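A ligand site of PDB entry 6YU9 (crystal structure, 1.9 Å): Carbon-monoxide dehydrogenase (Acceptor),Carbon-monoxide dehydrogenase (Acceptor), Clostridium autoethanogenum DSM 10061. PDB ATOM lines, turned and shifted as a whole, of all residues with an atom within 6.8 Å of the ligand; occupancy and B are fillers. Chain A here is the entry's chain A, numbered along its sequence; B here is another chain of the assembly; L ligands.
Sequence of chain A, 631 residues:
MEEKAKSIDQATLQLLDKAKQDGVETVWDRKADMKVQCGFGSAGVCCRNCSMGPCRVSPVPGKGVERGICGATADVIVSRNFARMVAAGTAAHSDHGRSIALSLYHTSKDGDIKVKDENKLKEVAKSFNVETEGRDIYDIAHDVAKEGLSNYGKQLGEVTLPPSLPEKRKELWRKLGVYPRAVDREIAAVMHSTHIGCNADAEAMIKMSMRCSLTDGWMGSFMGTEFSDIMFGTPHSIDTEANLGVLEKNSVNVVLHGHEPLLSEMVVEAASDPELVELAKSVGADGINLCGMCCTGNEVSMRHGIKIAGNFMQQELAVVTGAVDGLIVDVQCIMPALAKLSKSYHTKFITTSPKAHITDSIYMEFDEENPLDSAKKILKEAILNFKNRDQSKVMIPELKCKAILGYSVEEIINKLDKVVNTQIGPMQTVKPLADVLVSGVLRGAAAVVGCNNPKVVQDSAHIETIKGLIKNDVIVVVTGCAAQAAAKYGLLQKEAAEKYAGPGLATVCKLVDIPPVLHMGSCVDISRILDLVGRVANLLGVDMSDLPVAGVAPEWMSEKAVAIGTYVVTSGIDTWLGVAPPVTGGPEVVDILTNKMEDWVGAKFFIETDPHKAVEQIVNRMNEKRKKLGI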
ATOM      1  N   CYS A  46     -32.863 -14.615  -7.424  1.00  0.00           N
ATOM      2  CA  CYS A  46     -31.742 -13.718  -7.171  1.00  0.00           C
ATOM      3  C   CYS A  46     -31.693 -13.427  -5.658  1.00  0.00           C
ATOM      4  O   CYS A  46     -32.723 -13.124  -5.053  1.00  0.00           O
ATOM      5  CB  CYS A  46     -31.867 -12.430  -7.971  1.00  0.00           C
ATOM      6  SG  CYS A  46     -30.662 -11.178  -7.468  1.00  0.00           S
ATOM      7  N   CYS A  47     -30.483 -13.453  -5.069  1.00  0.00           N
ATOM      8  CA  CYS A  47     -30.322 -13.167  -3.659  1.00  0.00           C
ATOM      9  C   CYS A  47     -29.330 -12.060  -3.474  1.00  0.00           C
ATOM     10  O   CYS A  47     -28.282 -12.081  -4.108  1.00  0.00           O
ATOM     11  CB  CYS A  47     -29.898 -14.411  -2.877  1.00  0.00           C
ATOM     12  SG  CYS A  47     -29.796 -14.141  -1.073  1.00  0.00           S
ATOM     13  N   ARG A  48     -29.617 -11.122  -2.559  1.00  0.00           N
ATOM     14  CA  ARG A  48     -28.730 -10.012  -2.198  1.00  0.00           C
ATOM     15  C   ARG A  48     -28.660  -9.858  -0.665  1.00  0.00           C
ATOM     16  O   ARG A  48     -28.596  -8.740  -0.165  1.00  0.00           O
ATOM     17  CB  ARG A  48     -29.269  -8.711  -2.822  1.00  0.00           C
ATOM     18  CG  ARG A  48     -29.065  -8.581  -4.320  1.00  0.00           C
ATOM     19  CD  ARG A  48     -29.287  -7.173  -4.824  1.00  0.00           C
ATOM     20  NE  ARG A  48     -30.594  -6.640  -4.402  1.00  0.00           N
ATOM     21  CZ  ARG A  48     -31.650  -6.417  -5.188  1.00  0.00           C
ATOM     22  NH1 ARG A  48     -31.583  -6.685  -6.485  1.00  0.00           N
ATOM     23  NH2 ARG A  48     -32.771  -5.919  -4.685  1.00  0.00           N
ATOM     24  N   ASN A  49     -28.835 -10.956   0.091  1.00  0.00           N
ATOM     25  CA  ASN A  49     -28.890 -10.883   1.550  1.00  0.00           C
ATOM     26  C   ASN A  49     -27.511 -10.743   2.217  1.00  0.00           C
ATOM     27  O   ASN A  49     -27.440 -10.786   3.450  1.00  0.00           O
ATOM     28  CB  ASN A  49     -29.605 -12.091   2.107  1.00  0.00           C
ATOM     29  CG  ASN A  49     -31.087 -12.053   1.891  1.00  0.00           C
ATOM     30  OD1 ASN A  49     -31.593 -11.353   0.999  1.00  0.00           O
ATOM     31  ND2 ASN A  49     -31.815 -12.864   2.634  1.00  0.00           N
ATOM     32  N   CYS A  50     -26.459 -10.556   1.432  1.00  0.00           N
ATOM     33  CA  CYS A  50     -25.114 -10.378   2.027  1.00  0.00           C
ATOM     34  C   CYS A  50     -24.160  -9.907   0.927  1.00  0.00           C
ATOM     35  O   CYS A  50     -24.477 -10.070  -0.250  1.00  0.00           O
ATOM     36  CB  CYS A  50     -24.617 -11.636   2.737  1.00  0.00           C
ATOM     37  SG  CYS A  50     -23.760 -12.789   1.654  1.00  0.00           S
ATOM     38  N   SER A  51     -23.016  -9.339   1.326  1.00  0.00           N
ATOM     39  CA  SER A  51     -22.095  -8.828   0.349  1.00  0.00           C
ATOM     40  C   SER A  51     -21.174  -9.912  -0.180  1.00  0.00           C
ATOM     41  O   SER A  51     -20.299  -9.573  -0.961  1.00  0.00           O
ATOM     42  CB  SER A  51     -21.329  -7.622   0.889  1.00  0.00           C
ATOM     43  OG  SER A  51     -20.467  -8.028   1.942  1.00  0.00           O
ATOM     44  N   MET A  52     -21.418 -11.221   0.079  1.00  0.00           N
ATOM     45  CA  MET A  52     -20.734 -12.257  -0.719  1.00  0.00           C
ATOM     46  C   MET A  52     -21.463 -12.236  -2.109  1.00  0.00           C
ATOM     47  O   MET A  52     -20.851 -12.587  -3.118  1.00  0.00           O
ATOM     48  CB  MET A  52     -20.841 -13.669  -0.133  1.00  0.00           C
ATOM     49  CG  MET A  52     -20.100 -13.817   1.088  1.00  0.00           C
ATOM     50  SD  MET A  52     -19.734 -15.471   1.702  1.00  0.00           S
ATOM     51  CE  MET A  52     -21.367 -16.098   1.981  1.00  0.00           C
ATOM     52  N   GLY A  53     -22.753 -11.850  -2.120  1.00  0.00           N
ATOM     53  CA  GLY A  53     -23.563 -11.740  -3.324  1.00  0.00           C
ATOM     54  C   GLY A  53     -23.263 -10.459  -4.077  1.00  0.00           C
ATOM     55  O   GLY A  53     -22.299  -9.759  -3.772  1.00  0.00           O
ATOM     56  N   PRO A  54     -24.039 -10.132  -5.116  1.00  0.00           N
ATOM     57  CA  PRO A  54     -25.280 -10.814  -5.539  1.00  0.00           C
ATOM     58  C   PRO A  54     -25.112 -12.264  -6.015  1.00  0.00           C
ATOM     59  O   PRO A  54     -24.095 -12.630  -6.613  1.00  0.00           O
ATOM     60  CB  PRO A  54     -25.851  -9.897  -6.633  1.00  0.00           C
ATOM     61  CG  PRO A  54     -25.036  -8.670  -6.691  1.00  0.00           C
ATOM     62  CD  PRO A  54     -23.761  -8.912  -5.900  1.00  0.00           C
ATOM     63  N   CYS A  55     -26.116 -13.099  -5.727  1.00  0.00           N
ATOM     64  CA  CYS A  55     -26.154 -14.491  -6.143  1.00  0.00           C
ATOM     65  C   CYS A  55     -27.380 -14.677  -7.021  1.00  0.00           C
ATOM     66  O   CYS A  55     -28.357 -13.995  -6.834  1.00  0.00           O
ATOM     67  CB  CYS A  55     -26.217 -15.385  -4.920  1.00  0.00           C
ATOM     68  SG  CYS A  55     -24.656 -15.490  -4.000  1.00  0.00           S
ATOM     69  N   ARG A  56     -27.301 -15.530  -8.041  1.00  0.00           N
ATOM     70  CA  ARG A  56     -28.462 -15.894  -8.827  1.00  0.00           C
ATOM     71  C   ARG A  56     -28.290 -17.345  -9.158  1.00  0.00           C
ATOM     72  O   ARG A  56     -27.166 -17.772  -9.401  1.00  0.00           O
ATOM     73  CB  ARG A  56     -28.674 -15.046 -10.098  1.00  0.00           C
ATOM     74  CG  ARG A  56     -27.450 -14.784 -10.932  1.00  0.00           C
ATOM     75  CD  ARG A  56     -27.770 -13.839 -12.068  1.00  0.00           C
ATOM     76  NE  ARG A  56     -26.557 -13.277 -12.652  1.00  0.00           N
ATOM     77  CZ  ARG A  56     -26.525 -12.221 -13.474  1.00  0.00           C
ATOM     78  NH1 ARG A  56     -27.648 -11.594 -13.820  1.00  0.00           N
ATOM     79  NH2 ARG A  56     -25.356 -11.779 -13.939  1.00  0.00           N
ATOM     80  N   VAL A  57     -29.347 -18.136  -8.979  1.00  0.00           N
ATOM     81  CA  VAL A  57     -29.329 -19.555  -9.239  1.00  0.00           C
ATOM     82  C   VAL A  57     -30.345 -19.867 -10.336  1.00  0.00           C
ATOM     83  O   VAL A  57     -31.153 -19.014 -10.659  1.00  0.00           O
ATOM     84  CB  VAL A  57     -29.524 -20.424  -7.966  1.00  0.00           C
ATOM     85  CG1 VAL A  57     -28.496 -20.060  -6.895  1.00  0.00           C
ATOM     86  CG2 VAL A  57     -30.942 -20.313  -7.398  1.00  0.00           C
ATOM     87  N   ARG A  67     -26.596 -23.414  -6.522  1.00  0.00           N
ATOM     88  CA  ARG A  67     -26.507 -22.906  -5.155  1.00  0.00           C
ATOM     89  C   ARG A  67     -25.847 -21.539  -5.078  1.00  0.00           C
ATOM     90  O   ARG A  67     -25.036 -21.208  -5.943  1.00  0.00           O
ATOM     91  CB  ARG A  67     -25.788 -23.906  -4.237  1.00  0.00           C
ATOM     92  CG  ARG A  67     -26.599 -25.192  -4.081  1.00  0.00           C
ATOM     93  CD  ARG A  67     -25.868 -26.298  -3.380  1.00  0.00           C
ATOM     94  NE  ARG A  67     -26.193 -26.309  -1.953  1.00  0.00           N
ATOM     95  CZ  ARG A  67     -26.910 -27.241  -1.315  1.00  0.00           C
ATOM     96  NH1 ARG A  67     -27.385 -28.303  -1.973  1.00  0.00           N
ATOM     97  NH2 ARG A  67     -27.146 -27.126  -0.003  1.00  0.00           N
ATOM     98  N   GLY A  68     -26.260 -20.744  -4.094  1.00  0.00           N
ATOM     99  CA  GLY A  68     -25.667 -19.437  -3.808  1.00  0.00           C
ATOM    100  C   GLY A  68     -24.304 -19.640  -3.173  1.00  0.00           C
ATOM    101  O   GLY A  68     -23.972 -20.754  -2.761  1.00  0.00           O
ATOM    102  N   ILE A  69     -23.485 -18.601  -3.091  1.00  0.00           N
ATOM    103  CA  ILE A  69     -22.102 -18.770  -2.586  1.00  0.00           C
ATOM    104  C   ILE A  69     -22.057 -19.403  -1.210  1.00  0.00           C
ATOM    105  O   ILE A  69     -21.176 -20.211  -0.935  1.00  0.00           O
ATOM    106  CB  ILE A  69     -21.368 -17.421  -2.630  1.00  0.00           C
ATOM    107  CG1 ILE A  69     -21.238 -16.989  -4.137  1.00  0.00           C
ATOM    108  CG2 ILE A  69     -20.017 -17.475  -1.873  1.00  0.00           C
ATOM    109  CD1 ILE A  69     -20.898 -15.596  -4.366  1.00  0.00           C
ATOM    110  N   CYS A  70     -23.050 -19.082  -0.379  1.00  0.00           N
ATOM    111  CA  CYS A  70     -23.140 -19.619   1.004  1.00  0.00           C
ATOM    112  C   CYS A  70     -23.681 -21.061   0.989  1.00  0.00           C
ATOM    113  O   CYS A  70     -23.515 -21.759   2.000  1.00  0.00           O
ATOM    114  CB  CYS A  70     -24.049 -18.737   1.848  1.00  0.00           C
ATOM    115  SG  CYS A  70     -25.790 -18.841   1.352  1.00  0.00           S
ATOM    116  N   GLY A  71     -24.280 -21.461  -0.124  1.00  0.00           N
ATOM    117  CA  GLY A  71     -24.847 -22.799  -0.289  1.00  0.00           C
ATOM    118  C   GLY A  71     -26.354 -22.787  -0.456  1.00  0.00           C
ATOM    119  O   GLY A  71     -26.943 -23.816  -0.741  1.00  0.00           O
ATOM    120  N   ALA A  72     -27.014 -21.635  -0.266  1.00  0.00           N
ATOM    121  CA  ALA A  72     -28.468 -21.539  -0.379  1.00  0.00           C
ATOM    122  C   ALA A  72     -29.027 -22.087  -1.737  1.00  0.00           C
ATOM    123  O   ALA A  72     -28.611 -21.641  -2.816  1.00  0.00           O
ATOM    124  CB  ALA A  72     -28.918 -20.097  -0.146  1.00  0.00           C
ATOM    125  N   THR A  73     -29.991 -23.013  -1.686  1.00  0.00           N
ATOM    126  CA  THR A  73     -30.629 -23.497  -2.896  1.00  0.00           C
ATOM    127  C   THR A  73     -31.622 -22.433  -3.422  1.00  0.00           C
ATOM    128  O   THR A  73     -31.830 -21.412  -2.772  1.00  0.00           O
ATOM    129  CB  THR A  73     -31.384 -24.784  -2.568  1.00  0.00           C
ATOM    130  OG1 THR A  73     -32.447 -24.439  -1.646  1.00  0.00           O
ATOM    131  CG2 THR A  73     -30.471 -25.885  -2.039  1.00  0.00           C
ATOM    132  N   ILE A  77     -33.526 -19.426  -1.335  1.00  0.00           N
ATOM    133  CA  ILE A  77     -33.491 -18.046  -1.804  1.00  0.00           C
ATOM    134  C   ILE A  77     -34.915 -17.541  -2.059  1.00  0.00           C
ATOM    135  O   ILE A  77     -35.226 -16.432  -1.662  1.00  0.00           O
ATOM    136  CB  ILE A  77     -32.592 -17.923  -3.069  1.00  0.00           C
ATOM    137  CG1 ILE A  77     -31.116 -18.174  -2.695  1.00  0.00           C
ATOM    138  CG2 ILE A  77     -32.811 -16.532  -3.750  1.00  0.00           C
ATOM    139  CD1 ILE A  77     -30.190 -18.232  -3.772  1.00  0.00           C
ATOM    140  N   ARG A  80     -36.999 -17.128   1.457  1.00  0.00           N
ATOM    141  CA  ARG A  80     -36.545 -15.975   2.212  1.00  0.00           C
ATOM    142  C   ARG A  80     -37.024 -14.691   1.547  1.00  0.00           C
ATOM    143  O   ARG A  80     -37.530 -13.794   2.217  1.00  0.00           O
ATOM    144  CB  ARG A  80     -35.016 -15.963   2.315  1.00  0.00           C
ATOM    145  CG  ARG A  80     -34.469 -17.142   3.087  1.00  0.00           C
ATOM    146  CD  ARG A  80     -32.987 -16.983   3.386  1.00  0.00           C
ATOM    147  NE  ARG A  80     -32.192 -16.846   2.171  1.00  0.00           N
ATOM    148  CZ  ARG A  80     -30.868 -16.937   2.128  1.00  0.00           C
ATOM    149  NH1 ARG A  80     -30.164 -17.164   3.243  1.00  0.00           N
ATOM    150  NH2 ARG A  80     -30.232 -16.785   0.974  1.00  0.00           N
ATOM    151  N   THR A 194     -34.024 -14.659   7.853  1.00  0.00           N
ATOM    152  CA  THR A 194     -33.685 -14.558   6.436  1.00  0.00           C
ATOM    153  C   THR A 194     -32.228 -14.058   6.283  1.00  0.00           C
ATOM    154  O   THR A 194     -31.700 -14.038   5.173  1.00  0.00           O
ATOM    155  CB  THR A 194     -34.696 -13.672   5.701  1.00  0.00           C
ATOM    156  OG1 THR A 194     -34.670 -12.347   6.254  1.00  0.00           O
ATOM    157  CG2 THR A 194     -36.121 -14.242   5.738  1.00  0.00           C
ATOM    158  N   HIS A 195     -31.559 -13.724   7.400  1.00  0.00           N
ATOM    159  CA  HIS A 195     -30.174 -13.308   7.368  1.00  0.00           C
ATOM    160  C   HIS A 195     -29.300 -14.504   6.877  1.00  0.00           C
ATOM    161  O   HIS A 195     -29.735 -15.672   6.926  1.00  0.00           O
ATOM    162  CB  HIS A 195     -29.751 -12.850   8.778  1.00  0.00           C
ATOM    163  CG  HIS A 195     -28.378 -12.289   8.853  1.00  0.00           C
ATOM    164  ND1 HIS A 195     -27.254 -13.116   8.886  1.00  0.00           N
ATOM    165  CD2 HIS A 195     -27.977 -11.013   9.065  1.00  0.00           C
ATOM    166  CE1 HIS A 195     -26.216 -12.305   9.015  1.00  0.00           C
ATOM    167  NE2 HIS A 195     -26.592 -11.024   9.076  1.00  0.00           N
ATOM    168  N   ILE A 196     -28.110 -14.187   6.307  1.00  0.00           N
ATOM    169  CA  ILE A 196     -27.203 -15.218   5.818  1.00  0.00           C
ATOM    170  C   ILE A 196     -26.800 -16.199   6.945  1.00  0.00           C
ATOM    171  O   ILE A 196     -26.495 -15.777   8.069  1.00  0.00           O
ATOM    172  CB  ILE A 196     -25.966 -14.585   5.104  1.00  0.00           C
ATOM    173  CG1 ILE A 196     -25.165 -15.650   4.322  1.00  0.00           C
ATOM    174  CG2 ILE A 196     -25.079 -13.774   6.103  1.00  0.00           C
ATOM    175  CD1 ILE A 196     -24.009 -16.272   5.114  1.00  0.00           C
ATOM    176  N   GLY A 197     -26.863 -17.481   6.623  1.00  0.00           N
ATOM    177  CA  GLY A 197     -26.522 -18.567   7.512  1.00  0.00           C
ATOM    178  C   GLY A 197     -27.523 -18.858   8.598  1.00  0.00           C
ATOM    179  O   GLY A 197     -27.118 -19.272   9.681  1.00  0.00           O
ATOM    180  N   MET B  34     -20.378 -18.556  -9.583  1.00  0.00           N
ATOM    181  CA  MET B  34     -21.243 -17.391  -9.722  1.00  0.00           C
ATOM    182  C   MET B  34     -20.743 -16.440 -10.833  1.00  0.00           C
ATOM    183  O   MET B  34     -21.460 -15.528 -11.214  1.00  0.00           O
ATOM    184  CB  MET B  34     -21.342 -16.679  -8.348  1.00  0.00           C
ATOM    185  CG  MET B  34     -22.645 -15.918  -8.124  1.00  0.00           C
ATOM    186  SD  MET B  34     -24.157 -16.886  -8.437  1.00  0.00           S
ATOM    187  CE  MET B  34     -24.128 -17.993  -7.087  1.00  0.00           C
ATOM    188  N   GLN B  37     -20.700 -11.248 -11.062  1.00  0.00           N
ATOM    189  CA  GLN B  37     -21.889 -10.918 -10.306  1.00  0.00           C
ATOM    190  C   GLN B  37     -22.587  -9.714 -10.891  1.00  0.00           C
ATOM    191  O   GLN B  37     -21.943  -8.812 -11.412  1.00  0.00           O
ATOM    192  CB  GLN B  37     -21.508 -10.720  -8.849  1.00  0.00           C
ATOM    193  CG  GLN B  37     -21.057 -12.028  -8.243  1.00  0.00           C
ATOM    194  CD  GLN B  37     -20.626 -11.928  -6.818  1.00  0.00           C
ATOM    195  OE1 GLN B  37     -19.642 -11.254  -6.487  1.00  0.00           O
ATOM    196  NE2 GLN B  37     -21.369 -12.569  -5.928  1.00  0.00           N
ATOM    197  N   PRO B 336     -25.561 -23.067   4.660  1.00  0.00           N
ATOM    198  CA  PRO B 336     -26.417 -24.239   4.462  1.00  0.00           C
ATOM    199  C   PRO B 336     -25.752 -25.376   3.670  1.00  0.00           C
ATOM    200  O   PRO B 336     -26.214 -26.506   3.698  1.00  0.00           O
ATOM    201  CB  PRO B 336     -27.628 -23.694   3.717  1.00  0.00           C
ATOM    202  CG  PRO B 336     -27.404 -22.267   3.499  1.00  0.00           C
ATOM    203  CD  PRO B 336     -26.113 -21.853   4.039  1.00  0.00           C
ATOM    204  N   MET B 557     -19.046  -9.346   5.207  1.00  0.00           N
ATOM    205  CA  MET B 557     -19.976  -9.961   4.277  1.00  0.00           C
ATOM    206  C   MET B 557     -21.465  -9.795   4.750  1.00  0.00           C
ATOM    207  O   MET B 557     -22.341  -9.694   3.919  1.00  0.00           O
ATOM    208  CB  MET B 557     -19.600 -11.476   4.076  1.00  0.00           C
ATOM    209  CG  MET B 557     -20.746 -12.443   3.990  1.00  0.00           C
ATOM    210  SD  MET B 557     -21.581 -13.110   5.450  1.00  0.00           S
ATOM    211  CE  MET B 557     -20.207 -13.690   6.307  1.00  0.00           C
HETATM  212 FE1  LIG L   1     -25.508 -15.219  -1.871  1.00  0.00          FE
HETATM  213 FE2  LIG L   1     -26.130 -16.849   0.335  1.00  0.00          FE
HETATM  214 FE3  LIG L   1     -27.591 -14.744  -0.626  1.00  0.00          FE
HETATM  215 FE4  LIG L   1     -25.257 -14.038   0.538  1.00  0.00          FE
HETATM  216  S1  LIG L   1     -27.157 -14.962   1.426  1.00  0.00           S
HETATM  217  S2  LIG L   1     -26.283 -13.000  -1.469  1.00  0.00           S
HETATM  218  S3  LIG L   1     -24.002 -15.959  -0.423  1.00  0.00           S
HETATM  219  S4  LIG L   1     -27.199 -16.770  -1.756  1.00  0.00           S
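CA of Arg 48 touches S2 of the ligand, 3.9 Å away. Met 52 touches the ligand. CA of Gly 68 touches S4 of the ligand, at 3.7 Å. Ile 77 touches the ligand. CG1 of Ile 196 touches S1 of the ligand, at 3.6 Å. Hydrophobic or aromatic side chains that line the ligand: Met 52, Ile 69, Ile 77 and Ile 196. Within 4 Å of the ligand: Cys 47, Arg 48, Asn 49, Cys 50, Met 52, Gly 53, Cys 55, Gly 68, Ile 69, Cys 70, Ile 77, Arg 80 and Ile 196. The nearest printed residue that does not touch the ligand is Ala 72 (4.1 Å).
N of Cys 50 lies close to S2 of the ligand (3.8 Å). SG of Cys 50 binds FE4 of the ligand, 2.2 Å away. The backbone NH of Cys 70 lies close to a sulfur (S3) of the ligand (3.3 Å). The side-chain sulfur (SG) of Cys 70 binds an iron atom (FE2) of the ligand, 2.3 Å away. The side-chain sulfur (SG) of Cys 55 is bound to an iron atom (FE1) of the ligand (2.3 Å). SG of Cys 47 is bound to FE3 of the ligand (2.3 Å). S2 of the ligand lies close to N of Gly 53, at 3.8 Å. A sulfur (S1) of the ligand sits close to the guanidinium group (NH2) of Arg 80, at 3.6 Å. A sulfur (S2) of the ligand sits close to the backbone NH (N) of Asn 49 (3.6 Å). N of Ile 69 lies close to S3 of the ligand, at 3.8 Å.
The backbone NH (N) of Met 52 sits close to the side-chain sulfur (SG) of Cys 50 (3.2 Å). The side-chain sulfur (SG) of Cys 70 sits close to the backbone NH (N) of Ala 72. The backbone carbonyl oxygen (O) of Cys 55 sits at hydrogen-bond distance from the backbone NH (N) of Cys 47, at 2.8 Å. N of Ile 69 lies close to SG of Cys 55 (3.4 Å). The backbone carbonyl oxygen of Cys 55 lies close to the side-chain sulfur of Cys 46, at 3.7 Å. NH2 of Arg 80 sits close to SG of Cys 47 (3.4 Å). The backbone NH of Asn 49 lies close to the side-chain sulfur of Cys 47, at 3.5 Å. The side-chain amide nitrogen of Gln 37 of chain B is in hydrogen-bond range of the backbone carbonyl oxygen of Met 52, at 2.9 Å.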
